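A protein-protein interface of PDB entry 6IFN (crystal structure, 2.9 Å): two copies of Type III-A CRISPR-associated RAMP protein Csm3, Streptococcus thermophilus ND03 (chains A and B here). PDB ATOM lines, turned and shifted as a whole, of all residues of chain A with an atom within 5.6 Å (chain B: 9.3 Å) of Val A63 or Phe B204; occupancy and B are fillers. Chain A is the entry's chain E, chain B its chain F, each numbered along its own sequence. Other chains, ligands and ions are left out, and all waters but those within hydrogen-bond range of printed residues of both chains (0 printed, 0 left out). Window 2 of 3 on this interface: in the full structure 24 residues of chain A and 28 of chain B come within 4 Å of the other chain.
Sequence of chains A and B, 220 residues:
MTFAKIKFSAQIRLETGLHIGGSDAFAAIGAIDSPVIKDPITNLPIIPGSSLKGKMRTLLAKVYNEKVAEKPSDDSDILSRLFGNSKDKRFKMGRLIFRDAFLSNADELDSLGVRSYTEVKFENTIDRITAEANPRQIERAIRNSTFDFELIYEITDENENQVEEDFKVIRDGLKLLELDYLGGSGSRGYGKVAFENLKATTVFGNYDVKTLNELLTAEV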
ATOM      1  N   LEU A  59      -4.038 -23.843 -13.551  1.00  0.00           N
ATOM      2  CA  LEU A  59      -3.899 -24.472 -12.239  1.00  0.00           C
ATOM      3  C   LEU A  59      -4.688 -25.787 -12.226  1.00  0.00           C
ATOM      4  O   LEU A  59      -4.179 -26.833 -11.811  1.00  0.00           O
ATOM      5  CB  LEU A  59      -4.414 -23.524 -11.148  1.00  0.00           C
ATOM      6  CG  LEU A  59      -3.406 -22.506 -10.617  1.00  0.00           C
ATOM      7  CD1 LEU A  59      -4.053 -21.578  -9.603  1.00  0.00           C
ATOM      8  CD2 LEU A  59      -2.237 -23.228  -9.977  1.00  0.00           C
ATOM      9  N   LEU A  60      -5.938 -25.710 -12.698  1.00  0.00           N
ATOM     10  CA  LEU A  60      -6.859 -26.820 -12.616  1.00  0.00           C
ATOM     11  C   LEU A  60      -6.465 -27.929 -13.597  1.00  0.00           C
ATOM     12  O   LEU A  60      -6.815 -29.060 -13.391  1.00  0.00           O
ATOM     13  CB  LEU A  60      -8.268 -26.306 -12.874  1.00  0.00           C
ATOM     14  CG  LEU A  60      -8.950 -25.717 -11.640  1.00  0.00           C
ATOM     15  CD1 LEU A  60     -10.188 -24.933 -12.032  1.00  0.00           C
ATOM     16  CD2 LEU A  60      -9.301 -26.803 -10.640  1.00  0.00           C
ATOM     17  N   ALA A  61      -5.704 -27.607 -14.640  1.00  0.00           N
ATOM     18  CA  ALA A  61      -5.188 -28.631 -15.553  1.00  0.00           C
ATOM     19  C   ALA A  61      -4.228 -29.574 -14.823  1.00  0.00           C
ATOM     20  O   ALA A  61      -4.102 -30.721 -15.175  1.00  0.00           O
ATOM     21  CB  ALA A  61      -4.507 -27.996 -16.741  1.00  0.00           C
ATOM     22  N   LYS A  62      -3.541 -29.072 -13.800  1.00  0.00           N
ATOM     23  CA  LYS A  62      -2.548 -29.856 -13.044  1.00  0.00           C
ATOM     24  C   LYS A  62      -3.288 -30.897 -12.205  1.00  0.00           C
ATOM     25  O   LYS A  62      -2.762 -31.955 -11.970  1.00  0.00           O
ATOM     26  CB  LYS A  62      -1.625 -28.948 -12.211  1.00  0.00           C
ATOM     27  CG  LYS A  62      -0.828 -27.944 -13.044  1.00  0.00           C
ATOM     28  CD  LYS A  62       0.112 -27.018 -12.303  1.00  0.00           C
ATOM     29  CE  LYS A  62       0.796 -26.077 -13.283  1.00  0.00           C
ATOM     30  NZ  LYS A  62       1.971 -25.359 -12.728  1.00  0.00           N
ATOM     31  N   VAL A  63      -4.514 -30.586 -11.785  1.00  0.00           N
ATOM     32  CA  VAL A  63      -5.304 -31.531 -11.017  1.00  0.00           C
ATOM     33  C   VAL A  63      -6.088 -32.460 -11.954  1.00  0.00           C
ATOM     34  O   VAL A  63      -6.004 -33.673 -11.813  1.00  0.00           O
ATOM     35  CB  VAL A  63      -6.256 -30.806 -10.059  1.00  0.00           C
ATOM     36  CG1 VAL A  63      -7.174 -31.784  -9.351  1.00  0.00           C
ATOM     37  CG2 VAL A  63      -5.492 -29.968  -9.054  1.00  0.00           C
ATOM     38  N   TYR A  64      -6.865 -31.892 -12.885  1.00  0.00           N
ATOM     39  CA  TYR A  64      -7.984 -32.601 -13.484  1.00  0.00           C
ATOM     40  C   TYR A  64      -7.681 -33.147 -14.889  1.00  0.00           C
ATOM     41  O   TYR A  64      -8.528 -33.813 -15.462  1.00  0.00           O
ATOM     42  CB  TYR A  64      -9.208 -31.694 -13.557  1.00  0.00           C
ATOM     43  CG  TYR A  64      -9.966 -31.553 -12.266  1.00  0.00           C
ATOM     44  CD1 TYR A  64      -9.621 -30.583 -11.351  1.00  0.00           C
ATOM     45  CD2 TYR A  64     -11.030 -32.377 -11.942  1.00  0.00           C
ATOM     46  CE1 TYR A  64     -10.301 -30.433 -10.152  1.00  0.00           C
ATOM     47  CE2 TYR A  64     -11.718 -32.250 -10.743  1.00  0.00           C
ATOM     48  CZ  TYR A  64     -11.358 -31.268  -9.849  1.00  0.00           C
ATOM     49  OH  TYR A  64     -12.024 -31.113  -8.676  1.00  0.00           O
ATOM     50  N   ASN A  65      -6.494 -32.918 -15.442  1.00  0.00           N
ATOM     51  CA  ASN A  65      -6.167 -33.509 -16.737  1.00  0.00           C
ATOM     52  C   ASN A  65      -5.476 -34.847 -16.505  1.00  0.00           C
ATOM     53  O   ASN A  65      -4.384 -34.900 -15.952  1.00  0.00           O
ATOM     54  CB  ASN A  65      -5.268 -32.630 -17.606  1.00  0.00           C
ATOM     55  CG  ASN A  65      -6.037 -31.514 -18.275  1.00  0.00           C
ATOM     56  OD1 ASN A  65      -7.263 -31.520 -18.228  1.00  0.00           O
ATOM     57  ND2 ASN A  65      -5.332 -30.560 -18.874  1.00  0.00           N
ATOM     58  N   ASP A 172     -11.985 -25.970  -5.924  1.00  0.00           N
ATOM     59  CA  ASP A 172     -10.582 -26.319  -6.085  1.00  0.00           C
ATOM     60  C   ASP A 172      -9.859 -25.168  -6.784  1.00  0.00           C
ATOM     61  O   ASP A 172      -8.779 -24.782  -6.382  1.00  0.00           O
ATOM     62  CB  ASP A 172     -10.400 -27.632  -6.851  1.00  0.00           C
ATOM     63  CG  ASP A 172     -10.666 -28.873  -6.022  1.00  0.00           C
ATOM     64  OD1 ASP A 172     -10.888 -28.705  -4.794  1.00  0.00           O
ATOM     65  OD2 ASP A 172     -10.635 -29.991  -6.612  1.00  0.00           O
ATOM     66  N   LYS A 175      -9.348 -22.210  -4.380  1.00  0.00           N
ATOM     67  CA  LYS A 175      -8.358 -22.557  -3.350  1.00  0.00           C
ATOM     68  C   LYS A 175      -6.972 -22.551  -3.998  1.00  0.00           C
ATOM     69  O   LYS A 175      -6.038 -22.029  -3.420  1.00  0.00           O
ATOM     70  CB  LYS A 175      -8.651 -23.893  -2.651  1.00  0.00           C
ATOM     71  CG  LYS A 175      -7.996 -24.013  -1.273  1.00  0.00           C
ATOM     72  CD  LYS A 175      -8.114 -25.357  -0.590  1.00  0.00           C
ATOM     73  CE  LYS A 175      -8.896 -25.311   0.711  1.00  0.00           C
ATOM     74  NZ  LYS A 175      -9.229 -26.677   1.176  1.00  0.00           N
ATOM     75  N   LEU A 176      -6.865 -23.100  -5.213  1.00  0.00           N
ATOM     76  CA  LEU A 176      -5.588 -23.205  -5.887  1.00  0.00           C
ATOM     77  C   LEU A 176      -5.045 -21.808  -6.173  1.00  0.00           C
ATOM     78  O   LEU A 176      -3.836 -21.617  -6.071  1.00  0.00           O
ATOM     79  CB  LEU A 176      -5.720 -24.024  -7.170  1.00  0.00           C
ATOM     80  CG  LEU A 176      -5.749 -25.535  -6.967  1.00  0.00           C
ATOM     81  CD1 LEU A 176      -6.316 -26.225  -8.199  1.00  0.00           C
ATOM     82  CD2 LEU A 176      -4.365 -26.082  -6.642  1.00  0.00           C
ATOM     83  N   LEU A 179      -3.544 -20.658  -2.963  1.00  0.00           N
ATOM     84  CA  LEU A 179      -2.275 -21.345  -2.683  1.00  0.00           C
ATOM     85  C   LEU A 179      -1.309 -21.151  -3.849  1.00  0.00           C
ATOM     86  O   LEU A 179      -0.361 -21.918  -4.016  1.00  0.00           O
ATOM     87  CB  LEU A 179      -2.520 -22.844  -2.489  1.00  0.00           C
ATOM     88  CG  LEU A 179      -3.614 -23.211  -1.492  1.00  0.00           C
ATOM     89  CD1 LEU A 179      -3.931 -24.688  -1.589  1.00  0.00           C
ATOM     90  CD2 LEU A 179      -3.230 -22.812  -0.074  1.00  0.00           C
ATOM     91  N   THR B   2       1.661 -37.578  -7.713  1.00  0.00           N
ATOM     92  CA  THR B   2       0.374 -36.893  -7.897  1.00  0.00           C
ATOM     93  C   THR B   2       0.589 -35.367  -7.863  1.00  0.00           C
ATOM     94  O   THR B   2       1.702 -34.874  -8.045  1.00  0.00           O
ATOM     95  CB  THR B   2      -0.637 -37.413  -6.860  1.00  0.00           C
ATOM     96  OG1 THR B   2      -1.935 -37.031  -7.307  1.00  0.00           O
ATOM     97  CG2 THR B   2      -0.412 -36.892  -5.454  1.00  0.00           C
ATOM     98  N   PHE B   3      -0.493 -34.597  -7.650  1.00  0.00           N
ATOM     99  CA  PHE B   3      -0.389 -33.143  -7.401  1.00  0.00           C
ATOM    100  C   PHE B   3      -0.669 -32.825  -5.926  1.00  0.00           C
ATOM    101  O   PHE B   3      -1.617 -33.363  -5.336  1.00  0.00           O
ATOM    102  CB  PHE B   3      -1.352 -32.346  -8.285  1.00  0.00           C
ATOM    103  CG  PHE B   3      -1.296 -30.861  -8.069  1.00  0.00           C
ATOM    104  CD1 PHE B   3      -0.339 -30.100  -8.710  1.00  0.00           C
ATOM    105  CD2 PHE B   3      -2.202 -30.216  -7.243  1.00  0.00           C
ATOM    106  CE1 PHE B   3      -0.258 -28.734  -8.501  1.00  0.00           C
ATOM    107  CE2 PHE B   3      -2.129 -28.847  -7.043  1.00  0.00           C
ATOM    108  CZ  PHE B   3      -1.157 -28.112  -7.670  1.00  0.00           C
ATOM    109  N   ALA B   4       0.150 -31.931  -5.358  1.00  0.00           N
ATOM    110  CA  ALA B   4      -0.046 -31.426  -4.003  1.00  0.00           C
ATOM    111  C   ALA B   4       0.792 -30.160  -3.774  1.00  0.00           C
ATOM    112  O   ALA B   4       1.817 -29.948  -4.438  1.00  0.00           O
ATOM    113  CB  ALA B   4       0.315 -32.482  -2.995  1.00  0.00           C
ATOM    114  N   LYS B   5       0.337 -29.341  -2.811  1.00  0.00           N
ATOM    115  CA  LYS B   5       1.003 -28.109  -2.429  1.00  0.00           C
ATOM    116  C   LYS B   5       1.271 -28.116  -0.924  1.00  0.00           C
ATOM    117  O   LYS B   5       0.316 -28.226  -0.127  1.00  0.00           O
ATOM    118  CB  LYS B   5       0.156 -26.893  -2.801  1.00  0.00           C
ATOM    119  CG  LYS B   5       0.366 -26.429  -4.227  1.00  0.00           C
ATOM    120  CD  LYS B   5      -0.127 -25.028  -4.481  1.00  0.00           C
ATOM    121  CE  LYS B   5       0.252 -24.543  -5.867  1.00  0.00           C
ATOM    122  NZ  LYS B   5       1.674 -24.122  -5.925  1.00  0.00           N
ATOM    123  N   ILE B   6       2.568 -27.974  -0.586  1.00  0.00           N
ATOM    124  CA  ILE B   6       3.059 -27.897   0.782  1.00  0.00           C
ATOM    125  C   ILE B   6       3.471 -26.458   1.095  1.00  0.00           C
ATOM    126  O   ILE B   6       4.239 -25.858   0.336  1.00  0.00           O
ATOM    127  CB  ILE B   6       4.227 -28.870   1.017  1.00  0.00           C
ATOM    128  CG1 ILE B   6       3.836 -30.286   0.611  1.00  0.00           C
ATOM    129  CG2 ILE B   6       4.672 -28.823   2.470  1.00  0.00           C
ATOM    130  CD1 ILE B   6       4.398 -30.707  -0.700  1.00  0.00           C
ATOM    131  N   LYS B   7       2.981 -25.955   2.237  1.00  0.00           N
ATOM    132  CA  LYS B   7       3.289 -24.633   2.732  1.00  0.00           C
ATOM    133  C   LYS B   7       4.316 -24.723   3.869  1.00  0.00           C
ATOM    134  O   LYS B   7       4.014 -25.227   4.957  1.00  0.00           O
ATOM    135  CB  LYS B   7       2.010 -23.962   3.227  1.00  0.00           C
ATOM    136  CG  LYS B   7       2.225 -22.773   4.147  1.00  0.00           C
ATOM    137  CD  LYS B   7       0.927 -22.125   4.546  1.00  0.00           C
ATOM    138  CE  LYS B   7       1.103 -21.085   5.633  1.00  0.00           C
ATOM    139  NZ  LYS B   7      -0.196 -20.573   6.124  1.00  0.00           N
ATOM    140  N   ILE B 152       5.935 -21.837  -0.722  1.00  0.00           N
ATOM    141  CA  ILE B 152       5.049 -22.860  -1.266  1.00  0.00           C
ATOM    142  C   ILE B 152       5.840 -23.781  -2.193  1.00  0.00           C
ATOM    143  O   ILE B 152       6.554 -23.306  -3.074  1.00  0.00           O
ATOM    144  CB  ILE B 152       3.885 -22.229  -2.037  1.00  0.00           C
ATOM    145  CG1 ILE B 152       3.095 -21.245  -1.172  1.00  0.00           C
ATOM    146  CG2 ILE B 152       3.027 -23.327  -2.657  1.00  0.00           C
ATOM    147  CD1 ILE B 152       2.488 -21.857   0.067  1.00  0.00           C
ATOM    148  N   TYR B 153       5.681 -25.092  -1.977  1.00  0.00           N
ATOM    149  CA  TYR B 153       6.333 -26.102  -2.790  1.00  0.00           C
ATOM    150  C   TYR B 153       5.264 -26.948  -3.485  1.00  0.00           C
ATOM    151  O   TYR B 153       4.257 -27.320  -2.853  1.00  0.00           O
ATOM    152  CB  TYR B 153       7.256 -26.995  -1.964  1.00  0.00           C
ATOM    153  CG  TYR B 153       7.958 -28.045  -2.783  1.00  0.00           C
ATOM    154  CD1 TYR B 153       9.031 -27.716  -3.595  1.00  0.00           C
ATOM    155  CD2 TYR B 153       7.551 -29.367  -2.751  1.00  0.00           C
ATOM    156  CE1 TYR B 153       9.702 -28.679  -4.338  1.00  0.00           C
ATOM    157  CE2 TYR B 153       8.206 -30.343  -3.489  1.00  0.00           C
ATOM    158  CZ  TYR B 153       9.274 -29.998  -4.304  1.00  0.00           C
ATOM    159  OH  TYR B 153       9.891 -30.980  -5.031  1.00  0.00           O
ATOM    160  N   GLU B 154       5.504 -27.242  -4.773  1.00  0.00           N
ATOM    161  CA  GLU B 154       4.526 -27.869  -5.644  1.00  0.00           C
ATOM    162  C   GLU B 154       5.079 -29.229  -6.085  1.00  0.00           C
ATOM    163  O   GLU B 154       6.134 -29.288  -6.716  1.00  0.00           O
ATOM    164  CB  GLU B 154       4.216 -26.960  -6.837  1.00  0.00           C
ATOM    165  CG  GLU B 154       2.904 -27.256  -7.550  1.00  0.00           C
ATOM    166  CD  GLU B 154       2.731 -26.594  -8.915  1.00  0.00           C
ATOM    167  OE1 GLU B 154       3.670 -26.639  -9.741  1.00  0.00           O
ATOM    168  OE2 GLU B 154       1.652 -26.007  -9.143  1.00  0.00           O
ATOM    169  N   ILE B 155       4.363 -30.306  -5.757  1.00  0.00           N
ATOM    170  CA  ILE B 155       4.731 -31.588  -6.287  1.00  0.00           C
ATOM    171  C   ILE B 155       3.834 -31.909  -7.483  1.00  0.00           C
ATOM    172  O   ILE B 155       2.625 -32.093  -7.321  1.00  0.00           O
ATOM    173  CB  ILE B 155       4.666 -32.712  -5.245  1.00  0.00           C
ATOM    174  CG1 ILE B 155       5.111 -32.265  -3.857  1.00  0.00           C
ATOM    175  CG2 ILE B 155       5.485 -33.888  -5.733  1.00  0.00           C
ATOM    176  CD1 ILE B 155       4.842 -33.324  -2.810  1.00  0.00           C
ATOM    177  N   THR B 156       4.486 -31.972  -8.655  1.00  0.00           N
ATOM    178  CA  THR B 156       4.001 -32.536  -9.894  1.00  0.00           C
ATOM    179  C   THR B 156       5.221 -33.221 -10.514  1.00  0.00           C
ATOM    180  O   THR B 156       6.339 -32.696 -10.360  1.00  0.00           O
ATOM    181  CB  THR B 156       3.445 -31.447 -10.830  1.00  0.00           C
ATOM    182  OG1 THR B 156       4.529 -30.673 -11.335  1.00  0.00           O
ATOM    183  CG2 THR B 156       2.506 -30.446 -10.188  1.00  0.00           C
ATOM    184  N   THR B 201       3.313 -28.019   6.016  1.00  0.00           N
ATOM    185  CA  THR B 201       1.895 -28.397   6.038  1.00  0.00           C
ATOM    186  C   THR B 201       1.435 -28.632   4.598  1.00  0.00           C
ATOM    187  O   THR B 201       1.699 -27.798   3.733  1.00  0.00           O
ATOM    188  CB  THR B 201       1.019 -27.311   6.675  1.00  0.00           C
ATOM    189  OG1 THR B 201       1.709 -26.728   7.783  1.00  0.00           O
ATOM    190  CG2 THR B 201      -0.331 -27.867   7.066  1.00  0.00           C
ATOM    191  N   THR B 202       0.773 -29.763   4.343  1.00  0.00           N
ATOM    192  CA  THR B 202       0.192 -30.004   3.037  1.00  0.00           C
ATOM    193  C   THR B 202      -1.171 -29.311   3.008  1.00  0.00           C
ATOM    194  O   THR B 202      -2.060 -29.697   3.747  1.00  0.00           O
ATOM    195  CB  THR B 202       0.094 -31.504   2.740  1.00  0.00           C
ATOM    196  OG1 THR B 202       1.389 -32.094   2.846  1.00  0.00           O
ATOM    197  CG2 THR B 202      -0.479 -31.773   1.368  1.00  0.00           C
ATOM    198  N   VAL B 203      -1.300 -28.275   2.176  1.00  0.00           N
ATOM    199  CA  VAL B 203      -2.519 -27.447   2.123  1.00  0.00           C
ATOM    200  C   VAL B 203      -3.339 -27.807   0.876  1.00  0.00           C
ATOM    201  O   VAL B 203      -4.469 -27.331   0.716  1.00  0.00           O
ATOM    202  CB  VAL B 203      -2.206 -25.936   2.156  1.00  0.00           C
ATOM    203  CG1 VAL B 203      -2.023 -25.415   3.572  1.00  0.00           C
ATOM    204  CG2 VAL B 203      -1.012 -25.580   1.277  1.00  0.00           C
ATOM    205  N   PHE B 204      -2.766 -28.624  -0.009  1.00  0.00           N
ATOM    206  CA  PHE B 204      -3.501 -29.146  -1.148  1.00  0.00           C
ATOM    207  C   PHE B 204      -2.952 -30.524  -1.525  1.00  0.00           C
ATOM    208  O   PHE B 204      -1.748 -30.750  -1.486  1.00  0.00           O
ATOM    209  CB  PHE B 204      -3.445 -28.181  -2.337  1.00  0.00           C
ATOM    210  CG  PHE B 204      -4.560 -28.379  -3.342  1.00  0.00           C
ATOM    211  CD1 PHE B 204      -5.804 -27.789  -3.150  1.00  0.00           C
ATOM    212  CD2 PHE B 204      -4.380 -29.176  -4.463  1.00  0.00           C
ATOM    213  CE1 PHE B 204      -6.837 -28.003  -4.046  1.00  0.00           C
ATOM    214  CE2 PHE B 204      -5.405 -29.364  -5.378  1.00  0.00           C
ATOM    215  CZ  PHE B 204      -6.635 -28.786  -5.161  1.00  0.00           C
ATOM    216  N   GLY B 205      -3.856 -31.422  -1.910  1.00  0.00           N
ATOM    217  CA  GLY B 205      -3.495 -32.800  -2.211  1.00  0.00           C
ATOM    218  C   GLY B 205      -3.237 -33.572  -0.935  1.00  0.00           C
ATOM    219  O   GLY B 205      -3.684 -33.172   0.119  1.00  0.00           O
ATOM    220  N   ASN B 206      -2.485 -34.665  -1.062  1.00  0.00           N
ATOM    221  CA  ASN B 206      -2.081 -35.474   0.069  1.00  0.00           C
ATOM    222  C   ASN B 206      -0.567 -35.709  -0.029  1.00  0.00           C
ATOM    223  O   ASN B 206      -0.052 -36.174  -1.067  1.00  0.00           O
ATOM    224  CB  ASN B 206      -2.848 -36.802   0.125  1.00  0.00           C
ATOM    225  CG  ASN B 206      -4.307 -36.618   0.470  1.00  0.00           C
ATOM    226  OD1 ASN B 206      -4.643 -36.067   1.518  1.00  0.00           O
ATOM    227  ND2 ASN B 206      -5.180 -37.046  -0.422  1.00  0.00           N
ATOM    228  N   TYR B 207       0.143 -35.357   1.048  1.00  0.00           N
ATOM    229  CA  TYR B 207       1.526 -35.746   1.248  1.00  0.00           C
ATOM    230  C   TYR B 207       1.817 -35.858   2.744  1.00  0.00           C
ATOM    231  O   TYR B 207       1.210 -35.157   3.565  1.00  0.00           O
ATOM    232  CB  TYR B 207       2.495 -34.753   0.616  1.00  0.00           C
ATOM    233  CG  TYR B 207       3.854 -35.347   0.374  1.00  0.00           C
ATOM    234  CD1 TYR B 207       4.109 -36.061  -0.788  1.00  0.00           C
ATOM    235  CD2 TYR B 207       4.874 -35.224   1.305  1.00  0.00           C
ATOM    236  CE1 TYR B 207       5.353 -36.610  -1.041  1.00  0.00           C
ATOM    237  CE2 TYR B 207       6.123 -35.778   1.074  1.00  0.00           C
ATOM    238  CZ  TYR B 207       6.360 -36.469  -0.103  1.00  0.00           C
ATOM    239  OH  TYR B 207       7.575 -37.028  -0.356  1.00  0.00           O
ATOM    240  N   ASP B 208       2.760 -36.754   3.074  1.00  0.00           N
ATOM    241  CA  ASP B 208       3.141 -37.053   4.434  1.00  0.00           C
ATOM    242  C   ASP B 208       4.372 -36.229   4.820  1.00  0.00           C
ATOM    243  O   ASP B 208       5.473 -36.387   4.259  1.00  0.00           O
ATOM    244  CB  ASP B 208       3.467 -38.532   4.628  1.00  0.00           C
ATOM    245  CG  ASP B 208       4.033 -38.815   6.011  1.00  0.00           C
ATOM    246  OD1 ASP B 208       3.218 -38.868   6.956  1.00  0.00           O
ATOM    247  OD2 ASP B 208       5.284 -38.927   6.136  1.00  0.00           O
ATOM    248  N   VAL B 209       4.174 -35.387   5.836  1.00  0.00           N
ATOM    249  CA  VAL B 209       5.143 -34.373   6.223  1.00  0.00           C
ATOM    250  C   VAL B 209       5.855 -34.791   7.515  1.00  0.00           C
ATOM    251  O   VAL B 209       6.852 -34.194   7.842  1.00  0.00           O
ATOM    252  CB  VAL B 209       4.476 -32.988   6.373  1.00  0.00           C
ATOM    253  CG1 VAL B 209       4.201 -32.343   5.023  1.00  0.00           C
ATOM    254  CG2 VAL B 209       3.197 -33.038   7.204  1.00  0.00           C
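The backbone carbonyl oxygen (O) of Lys B5 sits at hydrogen-bond distance from the backbone NH (N) of Val B203. The side-chain amino group (NZ) of Lys B5 lies within salt-bridge range of the side-chain carboxylate (OE2) of Glu B154 (3.7 Å). The backbone carbonyl oxygen (O) of Phe B204 lies within hydrogen-bond range of the backbone NH (N) of Lys B5 (2.8 Å).
NZ of Lys A62 lies within salt-bridge range of OE2 of Glu B154, 3.7 Å away.
Hydrophobic or aromatic side chains of chain A that line the printed part of chain B: Val A63, Leu A176 and Leu A179. Hydrophobic or aromatic side chains of chain B within 4 Å of the printed part of chain A: Phe B3, Ile B152, Val B203 and Phe B204. Among the printed residues, 10 pairs touch across the chains.
Of chain B, only Phe B3 and Phe B204 come within 4 Å of Val A63. Of the printed residues of chain B, Leu A176 touches Phe B3 (3.6 Å) and Phe B204 (3.7 Å). Printed residues of chain A within 4 Å of Phe B3: Lys A62 (3.9 Å), Val A63 (3.8 Å) and Leu A176 (3.6 Å). Of the printed residues of chain A, Lys B5 touches Leu A179. Phe B204 touches three residues of chain A.
No position is printed for both chains. Of the 10 pairs that touch across the chains among the printed residues, none has its exchanged pair printed and touching as well.
Lys A62 touches Phe B3. Val A63 touches Phe B3 (CG2 to CD2, 3.8 Å). Val A63 touches Phe B204. Phe B3 touches Leu A176 (CE2 to CD2, 3.6 Å). Leu A176 touches Phe B204. Leu A179 touches Lys B5 (O to CD, 3.2 Å). Leu A179 touches Ile B152. CD1 of Leu A179 touches O of Val B203, at 3.5 Å. CB of Phe B204 touches CD1 of Leu A179, 3.6 Å away.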
